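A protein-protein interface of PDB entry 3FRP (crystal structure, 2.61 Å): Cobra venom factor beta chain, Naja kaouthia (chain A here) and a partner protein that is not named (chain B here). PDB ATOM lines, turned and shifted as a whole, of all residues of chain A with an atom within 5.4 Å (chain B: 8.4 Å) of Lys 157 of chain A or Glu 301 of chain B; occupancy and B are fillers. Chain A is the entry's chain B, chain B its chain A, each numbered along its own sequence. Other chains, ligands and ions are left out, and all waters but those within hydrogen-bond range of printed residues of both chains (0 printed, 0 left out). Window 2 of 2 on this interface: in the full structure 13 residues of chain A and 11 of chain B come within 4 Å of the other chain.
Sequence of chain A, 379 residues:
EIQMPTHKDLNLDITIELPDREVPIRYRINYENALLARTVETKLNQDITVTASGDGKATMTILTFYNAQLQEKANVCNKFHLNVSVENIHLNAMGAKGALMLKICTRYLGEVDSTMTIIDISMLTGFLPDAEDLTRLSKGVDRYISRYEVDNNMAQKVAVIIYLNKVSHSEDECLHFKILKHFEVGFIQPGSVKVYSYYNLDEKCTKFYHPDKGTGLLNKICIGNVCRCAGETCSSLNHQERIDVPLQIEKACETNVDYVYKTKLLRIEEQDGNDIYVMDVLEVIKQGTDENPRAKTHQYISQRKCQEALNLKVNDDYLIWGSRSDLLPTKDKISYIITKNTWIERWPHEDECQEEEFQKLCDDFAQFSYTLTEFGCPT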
ATOM      1  N   MET A 123      30.995  21.139  20.914  1.00  0.00           N
ATOM      2  CA  MET A 123      32.416  21.067  21.261  1.00  0.00           C
ATOM      3  C   MET A 123      33.153  20.131  20.334  1.00  0.00           C
ATOM      4  O   MET A 123      32.575  19.170  19.839  1.00  0.00           O
ATOM      5  CB  MET A 123      32.583  20.594  22.702  1.00  0.00           C
ATOM      6  CG  MET A 123      32.136  21.603  23.735  1.00  0.00           C
ATOM      7  SD  MET A 123      33.205  23.045  23.821  1.00  0.00           S
ATOM      8  CE  MET A 123      32.436  24.166  22.660  1.00  0.00           C
ATOM      9  N   PHE A 127      36.555  17.868  24.251  1.00  0.00           N
ATOM     10  CA  PHE A 127      36.762  19.255  24.630  1.00  0.00           C
ATOM     11  C   PHE A 127      35.599  19.731  25.440  1.00  0.00           C
ATOM     12  O   PHE A 127      34.470  19.254  25.288  1.00  0.00           O
ATOM     13  CB  PHE A 127      36.873  20.140  23.411  1.00  0.00           C
ATOM     14  CG  PHE A 127      38.262  20.288  22.895  1.00  0.00           C
ATOM     15  CD1 PHE A 127      39.039  21.379  23.265  1.00  0.00           C
ATOM     16  CD2 PHE A 127      38.794  19.354  22.028  1.00  0.00           C
ATOM     17  CE1 PHE A 127      40.321  21.538  22.777  1.00  0.00           C
ATOM     18  CE2 PHE A 127      40.069  19.506  21.531  1.00  0.00           C
ATOM     19  CZ  PHE A 127      40.836  20.606  21.907  1.00  0.00           C
ATOM     20  N   LEU A 128      35.875  20.701  26.295  1.00  0.00           N
ATOM     21  CA  LEU A 128      34.908  21.099  27.274  1.00  0.00           C
ATOM     22  C   LEU A 128      35.167  22.558  27.582  1.00  0.00           C
ATOM     23  O   LEU A 128      36.320  23.001  27.570  1.00  0.00           O
ATOM     24  CB  LEU A 128      35.068  20.216  28.517  1.00  0.00           C
ATOM     25  CG  LEU A 128      33.874  19.566  29.223  1.00  0.00           C
ATOM     26  CD1 LEU A 128      32.942  18.810  28.280  1.00  0.00           C
ATOM     27  CD2 LEU A 128      34.412  18.632  30.290  1.00  0.00           C
ATOM     28  N   PRO A 129      34.096  23.323  27.830  1.00  0.00           N
ATOM     29  CA  PRO A 129      34.236  24.740  28.130  1.00  0.00           C
ATOM     30  C   PRO A 129      34.845  25.038  29.509  1.00  0.00           C
ATOM     31  O   PRO A 129      34.484  24.415  30.512  1.00  0.00           O
ATOM     32  CB  PRO A 129      32.789  25.248  28.073  1.00  0.00           C
ATOM     33  CG  PRO A 129      32.028  24.189  27.338  1.00  0.00           C
ATOM     34  CD  PRO A 129      32.683  22.925  27.725  1.00  0.00           C
ATOM     35  N   SER A 146      21.662  27.831  30.011  1.00  0.00           N
ATOM     36  CA  SER A 146      21.117  26.836  30.923  1.00  0.00           C
ATOM     37  C   SER A 146      22.094  26.499  32.059  1.00  0.00           C
ATOM     38  O   SER A 146      23.309  26.676  31.914  1.00  0.00           O
ATOM     39  CB  SER A 146      20.784  25.560  30.147  1.00  0.00           C
ATOM     40  OG  SER A 146      19.596  25.713  29.400  1.00  0.00           O
ATOM     41  N   ARG A 147      21.553  26.023  33.186  1.00  0.00           N
ATOM     42  CA  ARG A 147      22.371  25.452  34.264  1.00  0.00           C
ATOM     43  C   ARG A 147      23.262  24.333  33.738  1.00  0.00           C
ATOM     44  O   ARG A 147      22.815  23.484  32.959  1.00  0.00           O
ATOM     45  CB  ARG A 147      21.500  24.880  35.383  1.00  0.00           C
ATOM     46  CG  ARG A 147      21.113  25.862  36.473  1.00  0.00           C
ATOM     47  CD  ARG A 147      19.767  26.554  36.155  1.00  0.00           C
ATOM     48  NE  ARG A 147      19.019  26.982  37.348  1.00  0.00           N
ATOM     49  CZ  ARG A 147      18.217  26.189  38.069  1.00  0.00           C
ATOM     50  NH1 ARG A 147      18.053  24.904  37.739  1.00  0.00           N
ATOM     51  NH2 ARG A 147      17.578  26.679  39.129  1.00  0.00           N
ATOM     52  N   TYR A 148      24.519  24.348  34.172  1.00  0.00           N
ATOM     53  CA  TYR A 148      25.466  23.274  33.907  1.00  0.00           C
ATOM     54  C   TYR A 148      26.252  22.896  35.168  1.00  0.00           C
ATOM     55  O   TYR A 148      26.477  23.727  36.053  1.00  0.00           O
ATOM     56  CB  TYR A 148      26.417  23.661  32.778  1.00  0.00           C
ATOM     57  CG  TYR A 148      27.073  25.018  32.943  1.00  0.00           C
ATOM     58  CD1 TYR A 148      26.505  26.160  32.388  1.00  0.00           C
ATOM     59  CD2 TYR A 148      28.268  25.159  33.635  1.00  0.00           C
ATOM     60  CE1 TYR A 148      27.104  27.412  32.536  1.00  0.00           C
ATOM     61  CE2 TYR A 148      28.876  26.403  33.777  1.00  0.00           C
ATOM     62  CZ  TYR A 148      28.289  27.524  33.226  1.00  0.00           C
ATOM     63  OH  TYR A 148      28.888  28.760  33.364  1.00  0.00           O
ATOM     64  N   ALA A 155      32.928  23.171  32.398  1.00  0.00           N
ATOM     65  CA  ALA A 155      31.474  23.142  32.253  1.00  0.00           C
ATOM     66  C   ALA A 155      31.085  21.821  31.628  1.00  0.00           C
ATOM     67  O   ALA A 155      31.627  21.442  30.588  1.00  0.00           O
ATOM     68  CB  ALA A 155      30.997  24.292  31.404  1.00  0.00           C
ATOM     69  N   GLN A 156      30.168  21.110  32.274  1.00  0.00           N
ATOM     70  CA  GLN A 156      29.857  19.744  31.856  1.00  0.00           C
ATOM     71  C   GLN A 156      28.764  19.695  30.768  1.00  0.00           C
ATOM     72  O   GLN A 156      27.645  19.193  30.974  1.00  0.00           O
ATOM     73  CB  GLN A 156      29.565  18.843  33.078  1.00  0.00           C
ATOM     74  CG  GLN A 156      30.025  17.372  32.890  1.00  0.00           C
ATOM     75  CD  GLN A 156      31.546  17.143  33.069  1.00  0.00           C
ATOM     76  OE1 GLN A 156      32.328  18.083  33.300  1.00  0.00           O
ATOM     77  NE2 GLN A 156      31.957  15.879  32.959  1.00  0.00           N
ATOM     78  N   LYS A 157      29.123  20.238  29.605  1.00  0.00           N
ATOM     79  CA  LYS A 157      28.223  20.341  28.460  1.00  0.00           C
ATOM     80  C   LYS A 157      29.009  20.353  27.172  1.00  0.00           C
ATOM     81  O   LYS A 157      29.954  21.132  27.027  1.00  0.00           O
ATOM     82  CB  LYS A 157      27.325  21.579  28.564  1.00  0.00           C
ATOM     83  CG  LYS A 157      26.139  21.345  29.483  1.00  0.00           C
ATOM     84  CD  LYS A 157      24.916  22.100  29.095  1.00  0.00           C
ATOM     85  CE  LYS A 157      23.730  21.514  29.811  1.00  0.00           C
ATOM     86  NZ  LYS A 157      22.560  22.426  29.720  1.00  0.00           N
ATOM     87  N   VAL A 158      28.627  19.470  26.249  1.00  0.00           N
ATOM     88  CA  VAL A 158      29.279  19.387  24.937  1.00  0.00           C
ATOM     89  C   VAL A 158      28.547  20.234  23.901  1.00  0.00           C
ATOM     90  O   VAL A 158      29.167  20.765  22.977  1.00  0.00           O
ATOM     91  CB  VAL A 158      29.395  17.942  24.445  1.00  0.00           C
ATOM     92  CG1 VAL A 158      28.058  17.260  24.512  1.00  0.00           C
ATOM     93  CG2 VAL A 158      29.913  17.901  23.038  1.00  0.00           C
ATOM     94  N   ALA A 159      27.230  20.336  24.054  1.00  0.00           N
ATOM     95  CA  ALA A 159      26.426  21.261  23.275  1.00  0.00           C
ATOM     96  C   ALA A 159      26.031  22.452  24.145  1.00  0.00           C
ATOM     97  O   ALA A 159      25.212  22.314  25.055  1.00  0.00           O
ATOM     98  CB  ALA A 159      25.195  20.562  22.743  1.00  0.00           C
ATOM     99  N   VAL A 160      26.626  23.609  23.873  1.00  0.00           N
ATOM    100  CA  VAL A 160      26.287  24.849  24.585  1.00  0.00           C
ATOM    101  C   VAL A 160      25.536  25.861  23.719  1.00  0.00           C
ATOM    102  O   VAL A 160      25.956  26.187  22.589  1.00  0.00           O
ATOM    103  CB  VAL A 160      27.529  25.531  25.194  1.00  0.00           C
ATOM    104  CG1 VAL A 160      28.660  25.575  24.193  1.00  0.00           C
ATOM    105  CG2 VAL A 160      27.199  26.943  25.673  1.00  0.00           C
ATOM    106  N   ILE A 161      24.437  26.371  24.270  1.00  0.00           N
ATOM    107  CA  ILE A 161      23.591  27.333  23.568  1.00  0.00           C
ATOM    108  C   ILE A 161      23.510  28.631  24.341  1.00  0.00           C
ATOM    109  O   ILE A 161      23.131  28.631  25.512  1.00  0.00           O
ATOM    110  CB  ILE A 161      22.190  26.738  23.298  1.00  0.00           C
ATOM    111  CG1 ILE A 161      22.297  25.705  22.169  1.00  0.00           C
ATOM    112  CG2 ILE A 161      21.212  27.808  22.893  1.00  0.00           C
ATOM    113  CD1 ILE A 161      21.495  24.447  22.388  1.00  0.00           C
ATOM    114  N   TYR A 163      21.742  32.324  24.544  1.00  0.00           N
ATOM    115  CA  TYR A 163      20.607  33.130  24.068  1.00  0.00           C
ATOM    116  C   TYR A 163      20.840  34.617  24.205  1.00  0.00           C
ATOM    117  O   TYR A 163      21.175  35.104  25.283  1.00  0.00           O
ATOM    118  CB  TYR A 163      19.338  32.766  24.806  1.00  0.00           C
ATOM    119  CG  TYR A 163      19.000  31.304  24.714  1.00  0.00           C
ATOM    120  CD1 TYR A 163      18.141  30.826  23.731  1.00  0.00           C
ATOM    121  CD2 TYR A 163      19.537  30.398  25.621  1.00  0.00           C
ATOM    122  CE1 TYR A 163      17.841  29.472  23.658  1.00  0.00           C
ATOM    123  CE2 TYR A 163      19.234  29.071  25.561  1.00  0.00           C
ATOM    124  CZ  TYR A 163      18.391  28.601  24.590  1.00  0.00           C
ATOM    125  OH  TYR A 163      18.115  27.254  24.562  1.00  0.00           O
ATOM    126  N   PHE B 202       8.952  15.308  22.614  1.00  0.00           N
ATOM    127  CA  PHE B 202       8.133  15.776  23.746  1.00  0.00           C
ATOM    128  C   PHE B 202       6.803  16.438  23.410  1.00  0.00           C
ATOM    129  O   PHE B 202       6.663  17.058  22.373  1.00  0.00           O
ATOM    130  CB  PHE B 202       8.932  16.713  24.650  1.00  0.00           C
ATOM    131  CG  PHE B 202       9.416  17.988  23.994  1.00  0.00           C
ATOM    132  CD1 PHE B 202      10.396  17.973  23.020  1.00  0.00           C
ATOM    133  CD2 PHE B 202       8.973  19.211  24.450  1.00  0.00           C
ATOM    134  CE1 PHE B 202      10.883  19.151  22.461  1.00  0.00           C
ATOM    135  CE2 PHE B 202       9.451  20.411  23.903  1.00  0.00           C
ATOM    136  CZ  PHE B 202      10.405  20.376  22.907  1.00  0.00           C
ATOM    137  N   TYR B 229       8.945  14.686  27.934  1.00  0.00           N
ATOM    138  CA  TYR B 229       9.232  13.683  26.901  1.00  0.00           C
ATOM    139  C   TYR B 229       8.115  12.647  26.798  1.00  0.00           C
ATOM    140  O   TYR B 229       7.354  12.449  27.740  1.00  0.00           O
ATOM    141  CB  TYR B 229      10.550  12.979  27.187  1.00  0.00           C
ATOM    142  CG  TYR B 229      11.749  13.845  26.945  1.00  0.00           C
ATOM    143  CD1 TYR B 229      12.149  14.148  25.657  1.00  0.00           C
ATOM    144  CD2 TYR B 229      12.496  14.369  28.009  1.00  0.00           C
ATOM    145  CE1 TYR B 229      13.260  14.960  25.416  1.00  0.00           C
ATOM    146  CE2 TYR B 229      13.627  15.180  27.775  1.00  0.00           C
ATOM    147  CZ  TYR B 229      13.995  15.465  26.468  1.00  0.00           C
ATOM    148  OH  TYR B 229      15.089  16.250  26.187  1.00  0.00           O
ATOM    149  N   GLU B 234      11.056  14.963  32.436  1.00  0.00           N
ATOM    150  CA  GLU B 234      10.858  16.367  32.176  1.00  0.00           C
ATOM    151  C   GLU B 234      11.815  16.786  31.104  1.00  0.00           C
ATOM    152  O   GLU B 234      12.887  16.215  30.950  1.00  0.00           O
ATOM    153  CB  GLU B 234      11.141  17.186  33.425  1.00  0.00           C
ATOM    154  CG  GLU B 234      10.716  16.507  34.712  1.00  0.00           C
ATOM    155  CD  GLU B 234       9.271  16.752  35.071  1.00  0.00           C
ATOM    156  OE1 GLU B 234       9.026  17.086  36.254  1.00  0.00           O
ATOM    157  OE2 GLU B 234       8.386  16.609  34.196  1.00  0.00           O
ATOM    158  N   VAL B 235      11.411  17.793  30.357  1.00  0.00           N
ATOM    159  CA  VAL B 235      12.274  18.426  29.409  1.00  0.00           C
ATOM    160  C   VAL B 235      12.968  19.599  30.095  1.00  0.00           C
ATOM    161  O   VAL B 235      12.362  20.277  30.917  1.00  0.00           O
ATOM    162  CB  VAL B 235      11.443  18.919  28.231  1.00  0.00           C
ATOM    163  CG1 VAL B 235      12.300  19.697  27.255  1.00  0.00           C
ATOM    164  CG2 VAL B 235      10.757  17.734  27.564  1.00  0.00           C
ATOM    165  N   GLU B 236      14.240  19.809  29.764  1.00  0.00           N
ATOM    166  CA  GLU B 236      14.954  21.036  30.114  1.00  0.00           C
ATOM    167  C   GLU B 236      15.167  21.853  28.853  1.00  0.00           C
ATOM    168  O   GLU B 236      15.405  21.291  27.781  1.00  0.00           O
ATOM    169  CB  GLU B 236      16.322  20.728  30.728  1.00  0.00           C
ATOM    170  CG  GLU B 236      16.291  20.110  32.118  1.00  0.00           C
ATOM    171  CD  GLU B 236      15.815  21.067  33.183  1.00  0.00           C
ATOM    172  OE1 GLU B 236      16.358  22.199  33.279  1.00  0.00           O
ATOM    173  OE2 GLU B 236      14.895  20.672  33.921  1.00  0.00           O
ATOM    174  N   GLY B 237      15.089  23.177  28.990  1.00  0.00           N
ATOM    175  CA  GLY B 237      15.325  24.119  27.887  1.00  0.00           C
ATOM    176  C   GLY B 237      14.645  25.469  28.099  1.00  0.00           C
ATOM    177  O   GLY B 237      14.353  25.860  29.237  1.00  0.00           O
ATOM    178  N   VAL B 238      14.388  26.178  26.998  1.00  0.00           N
ATOM    179  CA  VAL B 238      13.798  27.519  27.044  1.00  0.00           C
ATOM    180  C   VAL B 238      12.569  27.616  26.143  1.00  0.00           C
ATOM    181  O   VAL B 238      12.418  26.834  25.216  1.00  0.00           O
ATOM    182  CB  VAL B 238      14.819  28.616  26.628  1.00  0.00           C
ATOM    183  CG1 VAL B 238      16.174  28.400  27.302  1.00  0.00           C
ATOM    184  CG2 VAL B 238      14.976  28.635  25.128  1.00  0.00           C
ATOM    185  N   ILE B 263      12.607  26.813  30.764  1.00  0.00           N
ATOM    186  CA  ILE B 263      11.826  25.655  31.189  1.00  0.00           C
ATOM    187  C   ILE B 263      12.702  24.770  32.087  1.00  0.00           C
ATOM    188  O   ILE B 263      13.564  24.019  31.616  1.00  0.00           O
ATOM    189  CB  ILE B 263      11.262  24.872  29.988  1.00  0.00           C
ATOM    190  CG1 ILE B 263      10.516  25.816  29.027  1.00  0.00           C
ATOM    191  CG2 ILE B 263      10.358  23.749  30.459  1.00  0.00           C
ATOM    192  CD1 ILE B 263       9.184  26.371  29.560  1.00  0.00           C
ATOM    193  N   VAL B 298       8.872  25.758  22.258  1.00  0.00           N
ATOM    194  CA  VAL B 298       9.794  25.167  23.236  1.00  0.00           C
ATOM    195  C   VAL B 298      10.945  24.442  22.554  1.00  0.00           C
ATOM    196  O   VAL B 298      10.755  23.685  21.617  1.00  0.00           O
ATOM    197  CB  VAL B 298       9.093  24.184  24.196  1.00  0.00           C
ATOM    198  CG1 VAL B 298      10.065  23.710  25.298  1.00  0.00           C
ATOM    199  CG2 VAL B 298       7.879  24.822  24.809  1.00  0.00           C
ATOM    200  N   MET B 299      12.138  24.685  23.064  1.00  0.00           N
ATOM    201  CA  MET B 299      13.365  24.099  22.558  1.00  0.00           C
ATOM    202  C   MET B 299      14.110  23.334  23.688  1.00  0.00           C
ATOM    203  O   MET B 299      14.269  23.861  24.805  1.00  0.00           O
ATOM    204  CB  MET B 299      14.232  25.225  21.994  1.00  0.00           C
ATOM    205  CG  MET B 299      15.470  24.762  21.301  1.00  0.00           C
ATOM    206  SD  MET B 299      16.532  26.141  20.817  1.00  0.00           S
ATOM    207  CE  MET B 299      17.935  25.210  20.186  1.00  0.00           C
ATOM    208  N   THR B 300      14.547  22.097  23.397  1.00  0.00           N
ATOM    209  CA  THR B 300      15.387  21.325  24.351  1.00  0.00           C
ATOM    210  C   THR B 300      16.740  22.020  24.600  1.00  0.00           C
ATOM    211  O   THR B 300      17.277  22.688  23.716  1.00  0.00           O
ATOM    212  CB  THR B 300      15.600  19.837  23.944  1.00  0.00           C
ATOM    213  OG1 THR B 300      16.314  19.761  22.712  1.00  0.00           O
ATOM    214  CG2 THR B 300      14.289  19.110  23.790  1.00  0.00           C
ATOM    215  N   GLU B 301      17.270  21.859  25.813  1.00  0.00           N
ATOM    216  CA  GLU B 301      18.514  22.514  26.246  1.00  0.00           C
ATOM    217  C   GLU B 301      19.696  22.192  25.351  1.00  0.00           C
ATOM    218  O   GLU B 301      20.638  22.977  25.255  1.00  0.00           O
ATOM    219  CB  GLU B 301      18.845  22.125  27.691  1.00  0.00           C
ATOM    220  CG  GLU B 301      19.524  20.738  27.874  1.00  0.00           C
ATOM    221  CD  GLU B 301      19.533  20.267  29.333  1.00  0.00           C
ATOM    222  OE1 GLU B 301      18.888  19.217  29.605  1.00  0.00           O
ATOM    223  OE2 GLU B 301      20.149  20.959  30.198  1.00  0.00           O
ATOM    224  N   SER B 302      19.642  21.021  24.721  1.00  0.00           N
ATOM    225  CA  SER B 302      20.702  20.556  23.848  1.00  0.00           C
ATOM    226  C   SER B 302      20.529  21.104  22.425  1.00  0.00           C
ATOM    227  O   SER B 302      21.447  20.999  21.595  1.00  0.00           O
ATOM    228  CB  SER B 302      20.672  19.036  23.787  1.00  0.00           C
ATOM    229  OG  SER B 302      19.444  18.616  23.193  1.00  0.00           O
ATOM    230  N   GLY B 303      19.348  21.651  22.132  1.00  0.00           N
ATOM    231  CA  GLY B 303      19.046  22.129  20.799  1.00  0.00           C
ATOM    232  C   GLY B 303      18.643  21.034  19.844  1.00  0.00           C
ATOM    233  O   GLY B 303      18.461  21.300  18.671  1.00  0.00           O
ATOM    234  N   SER B 304      18.490  19.809  20.343  1.00  0.00           N
ATOM    235  CA  SER B 304      18.093  18.644  19.502  1.00  0.00           C
ATOM    236  C   SER B 304      16.757  18.788  18.738  1.00  0.00           C
ATOM    237  O   SER B 304      16.678  18.443  17.561  1.00  0.00           O
ATOM    238  CB  SER B 304      18.116  17.314  20.292  1.00  0.00           C
ATOM    239  OG  SER B 304      17.402  17.377  21.527  1.00  0.00           O
ATOM    240  N   ASP B 305      15.710  19.260  19.407  1.00  0.00           N
ATOM    241  CA  ASP B 305      14.455  19.517  18.709  1.00  0.00           C
ATOM    242  C   ASP B 305      13.569  20.454  19.477  1.00  0.00           C
ATOM    243  O   ASP B 305      13.778  20.684  20.659  1.00  0.00           O
ATOM    244  CB  ASP B 305      13.694  18.226  18.300  1.00  0.00           C
ATOM    245  CG  ASP B 305      13.042  17.506  19.473  1.00  0.00           C
ATOM    246  OD1 ASP B 305      12.006  16.832  19.259  1.00  0.00           O
ATOM    247  OD2 ASP B 305      13.563  17.598  20.607  1.00  0.00           O
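The side-chain carboxylate (OE2) of Glu 301 of chain B lies within salt-bridge range of the side-chain amino group (NZ) of Lys 157 of chain A, 2.9 Å away.
The backbone carbonyl oxygen (O) of Glu 236 of chain B is in hydrogen-bond range of the backbone NH (N) of Glu 301 of chain B (2.8 Å). O of Val 238 of chain B lies within hydrogen-bond range of N of Met 299 of chain B, at 3.1 Å. The side-chain hydroxyl of Ser 302 of chain B lies within hydrogen-bond range of the side-chain hydroxyl of Thr 300 of chain B (3.4 Å). The side-chain hydroxyl (OG) of Ser 302 of chain B is in hydrogen-bond range of the side-chain hydroxyl (OG) of Ser 304 of chain B (2.9 Å). The backbone carbonyl oxygen (O) of Arg 147 of chain A is in hydrogen-bond range of the side-chain amino group (NZ) of Lys 157 of chain A (3.4 Å).
Ser 302 of chain B touches Ala 159 of chain A (O to CB, 3.9 Å). Glu 301 of chain B touches Ile 161 of chain A (O to CD1, 3.3 Å). Ile 161 of chain A touches Ser 302 of chain B (CD1 to C, 3.5 Å). Ile 161 of chain A touches Gly 303 of chain B (CD1 to N, 3.5 Å). Val 238 of chain B touches Tyr 163 of chain A.
Of the printed residues of chain B, Lys 157 of chain A touches Glu 301 (2.9 Å). Printed residues of chain B within 4 Å of Tyr 163 of chain A: Val 238 (3.3 Å). Printed residues of chain A within 4 Å of Val 238 of chain B: Tyr 163. Printed residues of chain A within 4 Å of Ser 302 of chain B: Ala 159 and Ile 161. Of the printed residues of chain A, Gly 303 of chain B touches Ile 161. The nearest residue of chain B that does not touch Lys 157 of chain A is Ser 302 of chain B (6.0 Å).
Hydrophobic or aromatic side chains of chain B that line the printed part of chain A: Val 238. Of the 15 printed residues of chain A, 4 touch a printed residue of chain B. Hydrophobic or aromatic side chains of chain A that line the printed part of chain B: Ala 159, Ile 161 and Tyr 163. Along chain A the printed residues that touch a printed residue of chain B span positions 157 to 163. Among the printed residues, 6 pairs touch across the chains. Among the printed residues, Asp or Glu carboxylates within 4 Å of a Lys or Arg side-chain nitrogen of the other chain: Lys 157 of chain A with Glu 301 of chain B (2.9 Å).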
